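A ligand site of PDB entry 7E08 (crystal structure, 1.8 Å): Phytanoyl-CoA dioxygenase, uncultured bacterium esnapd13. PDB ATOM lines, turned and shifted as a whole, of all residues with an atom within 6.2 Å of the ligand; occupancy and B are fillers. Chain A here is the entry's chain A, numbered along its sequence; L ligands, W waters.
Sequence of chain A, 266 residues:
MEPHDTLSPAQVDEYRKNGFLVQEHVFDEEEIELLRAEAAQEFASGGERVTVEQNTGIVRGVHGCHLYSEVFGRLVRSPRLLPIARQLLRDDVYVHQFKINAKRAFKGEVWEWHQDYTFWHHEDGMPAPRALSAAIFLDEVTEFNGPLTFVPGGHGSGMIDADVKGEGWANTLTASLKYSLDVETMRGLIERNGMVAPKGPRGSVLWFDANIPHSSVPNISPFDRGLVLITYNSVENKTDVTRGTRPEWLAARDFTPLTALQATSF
Lys 99 touches the ligand (CE to O2, 3.6 Å).
NE2 of His 114 touches C4 of the ligand, 3.6 Å away.
Phe 119 touches the ligand.
Hydrophobic or aromatic side chains that line the ligand: His 114, Phe 119 and Trp 120.
Of the 19 residues printed, 8 come within 4 Å of the ligand.
O1 of the ligand lies within salt-bridge range of NH2 of Arg 246 (2.8 Å).
The side-chain carboxylate of Asp 116 lies close to an oxygen (O2) of the ligand (2.9 Å).
The backbone carbonyl oxygen (O) of Thr 172 is in hydrogen-bond range of a nitrogen (N1) of the ligand, 2.9 Å away.
NE2 of Gln 97 lies within hydrogen-bond range of O1 of the ligand.
The indole nitrogen (NE1) of Trp 120 is in hydrogen-bond range of an oxygen (O1) of the ligand (3.1 Å).
The side-chain hydroxyl of Thr 172 lies within hydrogen-bond range of the guanidinium group of Arg 246.
The side-chain carboxylate (OD2) of Asp 124 is in salt-bridge range of the guanidinium group (NH2) of Arg 246.
The side-chain carboxylate (OD1) of Asp 116 lies close to a ring nitrogen (NE2) of His 214, 3.5 Å away.
The side-chain amide oxygen of Gln 97 sits at hydrogen-bond distance from the side-chain amino group of Lys 99.
The side-chain amide nitrogen (NE2) of Gln 97 lies within hydrogen-bond range of the backbone carbonyl oxygen (O) of Leu 250 (3.0 Å).
N of His 214 is in hydrogen-bond range of O of His 114 (2.7 Å).
Water W1 lies within hydrogen-bond range of ND2 of Asn 101 (2.8 Å) and O2 of the ligand (3.2 Å).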
ATOM      1  N   HIS A  96     -14.660   9.143 -19.725  1.00  0.00           N
ATOM      2  CA  HIS A  96     -13.270   8.785 -20.069  1.00  0.00           C
ATOM      3  C   HIS A  96     -13.126   8.523 -21.542  1.00  0.00           C
ATOM      4  O   HIS A  96     -12.158   8.948 -22.146  1.00  0.00           O
ATOM      5  CB  HIS A  96     -12.922   7.527 -19.280  1.00  0.00           C
ATOM      6  CG  HIS A  96     -11.576   6.967 -19.601  1.00  0.00           C
ATOM      7  ND1 HIS A  96     -10.424   7.723 -19.456  1.00  0.00           N
ATOM      8  CD2 HIS A  96     -11.212   5.830 -20.232  1.00  0.00           C
ATOM      9  CE1 HIS A  96      -9.399   7.058 -19.979  1.00  0.00           C
ATOM     10  NE2 HIS A  96      -9.857   5.894 -20.408  1.00  0.00           N
ATOM     11  N   GLN A  97     -14.095   7.818 -22.102  1.00  0.00           N
ATOM     12  CA  GLN A  97     -14.046   7.343 -23.488  1.00  0.00           C
ATOM     13  C   GLN A  97     -15.450   7.173 -24.041  1.00  0.00           C
ATOM     14  O   GLN A  97     -16.388   6.808 -23.314  1.00  0.00           O
ATOM     15  CB  GLN A  97     -13.328   5.911 -23.498  1.00  0.00           C
ATOM     16  CG  GLN A  97     -13.104   5.377 -24.921  1.00  0.00           C
ATOM     17  CD  GLN A  97     -12.258   4.075 -24.861  1.00  0.00           C
ATOM     18  OE1 GLN A  97     -12.738   2.948 -24.641  1.00  0.00           O
ATOM     19  NE2 GLN A  97     -10.996   4.299 -24.881  1.00  0.00           N
ATOM     20  N   LYS A  99     -17.216   5.585 -27.698  1.00  0.00           N
ATOM     21  CA  LYS A  99     -16.952   4.942 -29.030  1.00  0.00           C
ATOM     22  C   LYS A  99     -18.221   4.367 -29.565  1.00  0.00           C
ATOM     23  O   LYS A  99     -19.154   3.972 -28.840  1.00  0.00           O
ATOM     24  CB  LYS A  99     -15.824   3.916 -28.877  1.00  0.00           C
ATOM     25  CG  LYS A  99     -16.063   2.756 -27.946  1.00  0.00           C
ATOM     26  CD  LYS A  99     -14.778   1.924 -27.651  1.00  0.00           C
ATOM     27  CE  LYS A  99     -15.060   0.861 -26.584  1.00  0.00           C
ATOM     28  NZ  LYS A  99     -15.091   1.513 -25.226  1.00  0.00           N
ATOM     29  N   ASN A 101     -19.308   1.233 -32.007  1.00  0.00           N
ATOM     30  CA  ASN A 101     -18.833  -0.133 -32.553  1.00  0.00           C
ATOM     31  C   ASN A 101     -20.000  -0.720 -33.325  1.00  0.00           C
ATOM     32  O   ASN A 101     -20.971  -1.177 -32.717  1.00  0.00           O
ATOM     33  CB  ASN A 101     -18.406  -1.101 -31.397  1.00  0.00           C
ATOM     34  CG  ASN A 101     -17.071  -0.724 -30.745  1.00  0.00           C
ATOM     35  OD1 ASN A 101     -16.263   0.117 -31.263  1.00  0.00           O
ATOM     36  ND2 ASN A 101     -16.803  -1.350 -29.622  1.00  0.00           N
ATOM     37  N   TRP A 111     -13.695 -10.989 -31.342  1.00  0.00           N
ATOM     38  CA  TRP A 111     -12.912 -10.088 -30.421  1.00  0.00           C
ATOM     39  C   TRP A 111     -12.397 -10.829 -29.223  1.00  0.00           C
ATOM     40  O   TRP A 111     -13.230 -11.364 -28.386  1.00  0.00           O
ATOM     41  CB  TRP A 111     -13.724  -8.974 -29.817  1.00  0.00           C
ATOM     42  CG  TRP A 111     -14.066  -7.943 -30.742  1.00  0.00           C
ATOM     43  CD1 TRP A 111     -14.828  -8.069 -31.864  1.00  0.00           C
ATOM     44  CD2 TRP A 111     -13.744  -6.554 -30.616  1.00  0.00           C
ATOM     45  NE1 TRP A 111     -15.003  -6.842 -32.467  1.00  0.00           N
ATOM     46  CE2 TRP A 111     -14.340  -5.892 -31.723  1.00  0.00           C
ATOM     47  CE3 TRP A 111     -12.992  -5.810 -29.710  1.00  0.00           C
ATOM     48  CZ2 TRP A 111     -14.221  -4.512 -31.932  1.00  0.00           C
ATOM     49  CZ3 TRP A 111     -12.859  -4.428 -29.917  1.00  0.00           C
ATOM     50  CH2 TRP A 111     -13.485  -3.801 -31.024  1.00  0.00           C
ATOM     51  N   HIS A 114     -11.149  -9.997 -23.036  1.00  0.00           N
ATOM     52  CA  HIS A 114     -10.355  -8.916 -22.437  1.00  0.00           C
ATOM     53  C   HIS A 114     -11.163  -8.148 -21.384  1.00  0.00           C
ATOM     54  O   HIS A 114     -12.396  -8.363 -21.224  1.00  0.00           O
ATOM     55  CB  HIS A 114      -9.858  -7.911 -23.472  1.00  0.00           C
ATOM     56  CG  HIS A 114     -10.971  -7.113 -24.118  1.00  0.00           C
ATOM     57  ND1 HIS A 114     -11.888  -7.674 -24.991  1.00  0.00           N
ATOM     58  CD2 HIS A 114     -11.307  -5.805 -24.008  1.00  0.00           C
ATOM     59  CE1 HIS A 114     -12.716  -6.727 -25.423  1.00  0.00           C
ATOM     60  NE2 HIS A 114     -12.411  -5.598 -24.802  1.00  0.00           N
ATOM     61  N   GLN A 115     -10.404  -7.344 -20.638  1.00  0.00           N
ATOM     62  CA  GLN A 115     -10.966  -6.454 -19.565  1.00  0.00           C
ATOM     63  C   GLN A 115     -10.595  -5.052 -19.988  1.00  0.00           C
ATOM     64  O   GLN A 115      -9.445  -4.735 -20.232  1.00  0.00           O
ATOM     65  CB  GLN A 115     -10.325  -6.756 -18.183  1.00  0.00           C
ATOM     66  CG  GLN A 115     -10.745  -8.015 -17.534  1.00  0.00           C
ATOM     67  CD  GLN A 115      -9.897  -8.306 -16.294  1.00  0.00           C
ATOM     68  OE1 GLN A 115      -8.660  -8.347 -16.387  1.00  0.00           O
ATOM     69  NE2 GLN A 115     -10.558  -8.552 -15.171  1.00  0.00           N
ATOM     70  N   ASP A 116     -11.595  -4.139 -20.103  1.00  0.00           N
ATOM     71  CA  ASP A 116     -11.287  -2.758 -20.515  1.00  0.00           C
ATOM     72  C   ASP A 116     -10.326  -2.093 -19.559  1.00  0.00           C
ATOM     73  O   ASP A 116      -9.511  -1.247 -19.932  1.00  0.00           O
ATOM     74  CB  ASP A 116     -12.604  -1.887 -20.440  1.00  0.00           C
ATOM     75  CG  ASP A 116     -13.625  -2.210 -21.553  1.00  0.00           C
ATOM     76  OD1 ASP A 116     -13.224  -2.785 -22.569  1.00  0.00           O
ATOM     77  OD2 ASP A 116     -14.866  -1.951 -21.375  1.00  0.00           O
ATOM     78  N   TYR A 117     -10.509  -2.357 -18.278  1.00  0.00           N
ATOM     79  CA  TYR A 117      -9.653  -1.598 -17.301  1.00  0.00           C
ATOM     80  C   TYR A 117      -8.154  -1.793 -17.489  1.00  0.00           C
ATOM     81  O   TYR A 117      -7.340  -0.893 -17.316  1.00  0.00           O
ATOM     82  CB  TYR A 117     -10.075  -1.950 -15.873  1.00  0.00           C
ATOM     83  CG  TYR A 117      -9.139  -1.355 -14.817  1.00  0.00           C
ATOM     84  CD1 TYR A 117      -9.060   0.011 -14.646  1.00  0.00           C
ATOM     85  CD2 TYR A 117      -8.335  -2.181 -14.015  1.00  0.00           C
ATOM     86  CE1 TYR A 117      -8.197   0.569 -13.696  1.00  0.00           C
ATOM     87  CE2 TYR A 117      -7.465  -1.643 -13.043  1.00  0.00           C
ATOM     88  CZ  TYR A 117      -7.404  -0.250 -12.873  1.00  0.00           C
ATOM     89  OH  TYR A 117      -6.583   0.301 -11.928  1.00  0.00           O
ATOM     90  N   PHE A 119      -6.571  -1.813 -20.251  1.00  0.00           N
ATOM     91  CA  PHE A 119      -6.111  -0.819 -21.171  1.00  0.00           C
ATOM     92  C   PHE A 119      -6.066   0.539 -20.511  1.00  0.00           C
ATOM     93  O   PHE A 119      -5.167   1.297 -20.665  1.00  0.00           O
ATOM     94  CB  PHE A 119      -7.076  -0.672 -22.350  1.00  0.00           C
ATOM     95  CG  PHE A 119      -7.175  -1.896 -23.229  1.00  0.00           C
ATOM     96  CD1 PHE A 119      -7.852  -3.025 -22.800  1.00  0.00           C
ATOM     97  CD2 PHE A 119      -6.601  -1.892 -24.481  1.00  0.00           C
ATOM     98  CE1 PHE A 119      -7.941  -4.170 -23.593  1.00  0.00           C
ATOM     99  CE2 PHE A 119      -6.705  -3.019 -25.290  1.00  0.00           C
ATOM    100  CZ  PHE A 119      -7.371  -4.148 -24.830  1.00  0.00           C
ATOM    101  N   TRP A 120      -7.105   0.877 -19.778  1.00  0.00           N
ATOM    102  CA  TRP A 120      -7.207   2.257 -19.273  1.00  0.00           C
ATOM    103  C   TRP A 120      -6.127   2.448 -18.168  1.00  0.00           C
ATOM    104  O   TRP A 120      -5.582   3.497 -18.006  1.00  0.00           O
ATOM    105  CB  TRP A 120      -8.603   2.492 -18.702  1.00  0.00           C
ATOM    106  CG  TRP A 120      -9.682   2.380 -19.751  1.00  0.00           C
ATOM    107  CD1 TRP A 120      -9.533   2.610 -21.067  1.00  0.00           C
ATOM    108  CD2 TRP A 120     -11.025   2.013 -19.573  1.00  0.00           C
ATOM    109  NE1 TRP A 120     -10.690   2.384 -21.712  1.00  0.00           N
ATOM    110  CE2 TRP A 120     -11.626   2.002 -20.836  1.00  0.00           C
ATOM    111  CE3 TRP A 120     -11.781   1.691 -18.461  1.00  0.00           C
ATOM    112  CZ2 TRP A 120     -12.949   1.676 -21.025  1.00  0.00           C
ATOM    113  CZ3 TRP A 120     -13.101   1.335 -18.637  1.00  0.00           C
ATOM    114  CH2 TRP A 120     -13.675   1.319 -19.932  1.00  0.00           C
ATOM    115  N   GLU A 123      -2.527   2.125 -20.384  1.00  0.00           N
ATOM    116  CA  GLU A 123      -2.339   3.148 -21.402  1.00  0.00           C
ATOM    117  C   GLU A 123      -2.659   4.565 -20.939  1.00  0.00           C
ATOM    118  O   GLU A 123      -2.092   5.518 -21.460  1.00  0.00           O
ATOM    119  CB  GLU A 123      -3.224   2.855 -22.645  1.00  0.00           C
ATOM    120  CG  GLU A 123      -3.109   1.451 -23.257  1.00  0.00           C
ATOM    121  CD  GLU A 123      -1.704   1.197 -23.820  1.00  0.00           C
ATOM    122  OE1 GLU A 123      -1.294   2.075 -24.619  1.00  0.00           O
ATOM    123  OE2 GLU A 123      -1.051   0.172 -23.439  1.00  0.00           O
ATOM    124  N   ASP A 124      -3.635   4.702 -20.011  1.00  0.00           N
ATOM    125  CA  ASP A 124      -4.192   6.025 -19.700  1.00  0.00           C
ATOM    126  C   ASP A 124      -3.868   6.500 -18.292  1.00  0.00           C
ATOM    127  O   ASP A 124      -4.108   7.664 -17.993  1.00  0.00           O
ATOM    128  CB  ASP A 124      -5.732   6.018 -19.903  1.00  0.00           C
ATOM    129  CG  ASP A 124      -6.148   5.669 -21.315  1.00  0.00           C
ATOM    130  OD1 ASP A 124      -5.413   5.950 -22.282  1.00  0.00           O
ATOM    131  OD2 ASP A 124      -7.246   5.075 -21.463  1.00  0.00           O
ATOM    132  N   THR A 172      -4.978  -1.303 -29.656  1.00  0.00           N
ATOM    133  CA  THR A 172      -6.006  -1.211 -28.623  1.00  0.00           C
ATOM    134  C   THR A 172      -7.449  -1.174 -29.189  1.00  0.00           C
ATOM    135  O   THR A 172      -8.433  -1.295 -28.423  1.00  0.00           O
ATOM    136  CB  THR A 172      -5.760   0.067 -27.721  1.00  0.00           C
ATOM    137  OG1 THR A 172      -5.773   1.300 -28.494  1.00  0.00           O
ATOM    138  CG2 THR A 172      -4.427  -0.089 -26.964  1.00  0.00           C
ATOM    139  N   LEU A 173      -7.570  -0.881 -30.458  1.00  0.00           N
ATOM    140  CA  LEU A 173      -8.864  -0.714 -31.095  1.00  0.00           C
ATOM    141  C   LEU A 173      -9.192  -1.744 -32.156  1.00  0.00           C
ATOM    142  O   LEU A 173     -10.193  -1.658 -32.829  1.00  0.00           O
ATOM    143  CB  LEU A 173      -8.932   0.675 -31.715  1.00  0.00           C
ATOM    144  CG  LEU A 173      -8.492   1.868 -30.899  1.00  0.00           C
ATOM    145  CD1 LEU A 173      -8.610   3.096 -31.744  1.00  0.00           C
ATOM    146  CD2 LEU A 173      -9.391   1.944 -29.700  1.00  0.00           C
ATOM    147  N   LEU A 177      -6.136  -7.524 -30.192  1.00  0.00           N
ATOM    148  CA  LEU A 177      -6.001  -6.600 -29.079  1.00  0.00           C
ATOM    149  C   LEU A 177      -4.695  -6.708 -28.344  1.00  0.00           C
ATOM    150  O   LEU A 177      -4.165  -7.775 -28.168  1.00  0.00           O
ATOM    151  CB  LEU A 177      -7.096  -6.813 -28.048  1.00  0.00           C
ATOM    152  CG  LEU A 177      -8.489  -6.402 -28.381  1.00  0.00           C
ATOM    153  CD1 LEU A 177      -9.348  -6.644 -27.198  1.00  0.00           C
ATOM    154  CD2 LEU A 177      -8.451  -4.947 -28.760  1.00  0.00           C
ATOM    155  N   HIS A 214     -14.742  -9.690 -21.285  1.00  0.00           N
ATOM    156  CA  HIS A 214     -15.697  -9.809 -22.389  1.00  0.00           C
ATOM    157  C   HIS A 214     -15.083 -10.037 -23.752  1.00  0.00           C
ATOM    158  O   HIS A 214     -13.980  -9.739 -23.996  1.00  0.00           O
ATOM    159  CB  HIS A 214     -16.712  -8.598 -22.428  1.00  0.00           C
ATOM    160  CG  HIS A 214     -16.091  -7.273 -22.694  1.00  0.00           C
ATOM    161  ND1 HIS A 214     -15.403  -6.582 -21.737  1.00  0.00           N
ATOM    162  CD2 HIS A 214     -16.036  -6.500 -23.820  1.00  0.00           C
ATOM    163  CE1 HIS A 214     -14.912  -5.470 -22.264  1.00  0.00           C
ATOM    164  NE2 HIS A 214     -15.282  -5.392 -23.518  1.00  0.00           N
ATOM    165  N   ARG A 246      -2.315   8.473 -24.860  1.00  0.00           N
ATOM    166  CA  ARG A 246      -3.246   8.471 -26.003  1.00  0.00           C
ATOM    167  C   ARG A 246      -3.919   9.808 -26.194  1.00  0.00           C
ATOM    168  O   ARG A 246      -3.877  10.648 -25.342  1.00  0.00           O
ATOM    169  CB  ARG A 246      -4.213   7.358 -25.883  1.00  0.00           C
ATOM    170  CG  ARG A 246      -3.547   6.028 -25.650  1.00  0.00           C
ATOM    171  CD  ARG A 246      -4.481   4.880 -25.964  1.00  0.00           C
ATOM    172  NE  ARG A 246      -5.528   4.747 -24.950  1.00  0.00           N
ATOM    173  CZ  ARG A 246      -6.493   3.834 -24.960  1.00  0.00           C
ATOM    174  NH1 ARG A 246      -6.585   2.952 -25.971  1.00  0.00           N
ATOM    175  NH2 ARG A 246      -7.381   3.788 -23.946  1.00  0.00           N
ATOM    176  N   LEU A 250      -9.466   9.330 -27.275  1.00  0.00           N
ATOM    177  CA  LEU A 250      -9.512   8.062 -26.605  1.00  0.00           C
ATOM    178  C   LEU A 250      -9.535   8.078 -25.090  1.00  0.00           C
ATOM    179  O   LEU A 250     -10.009   7.115 -24.450  1.00  0.00           O
ATOM    180  CB  LEU A 250      -8.304   7.148 -27.019  1.00  0.00           C
ATOM    181  CG  LEU A 250      -8.234   6.784 -28.516  1.00  0.00           C
ATOM    182  CD1 LEU A 250      -6.985   5.912 -28.815  1.00  0.00           C
ATOM    183  CD2 LEU A 250      -9.507   5.963 -28.804  1.00  0.00           C
HETATM  184  N1  LIG L   1     -10.528  -0.978 -26.489  1.00  0.00           N
HETATM  185  C1  LIG L   1     -10.720   0.014 -25.387  1.00  0.00           C
HETATM  186  C2  LIG L   1      -9.511   0.901 -25.232  1.00  0.00           C
HETATM  187  O1  LIG L   1      -9.410   1.878 -24.485  1.00  0.00           O
HETATM  188  C3  LIG L   1     -11.086  -0.865 -24.197  1.00  0.00           C
HETATM  189  C4  LIG L   1     -11.682  -2.122 -24.867  1.00  0.00           C
HETATM  190  C5  LIG L   1     -10.788  -2.290 -26.080  1.00  0.00           C
HETATM  191  O2  LIG L   1     -13.054  -1.895 -25.338  1.00  0.00           O
HETATM  192  O3  LIG L   1      -8.547   0.702 -25.959  1.00  0.00           O
HETATM  193  O   HOH W   1     -14.737  -2.307 -27.999  1.00  0.00           O
HETATM  194  O   HOH W   2     -12.523  -0.705 -28.423  1.00  0.00           O
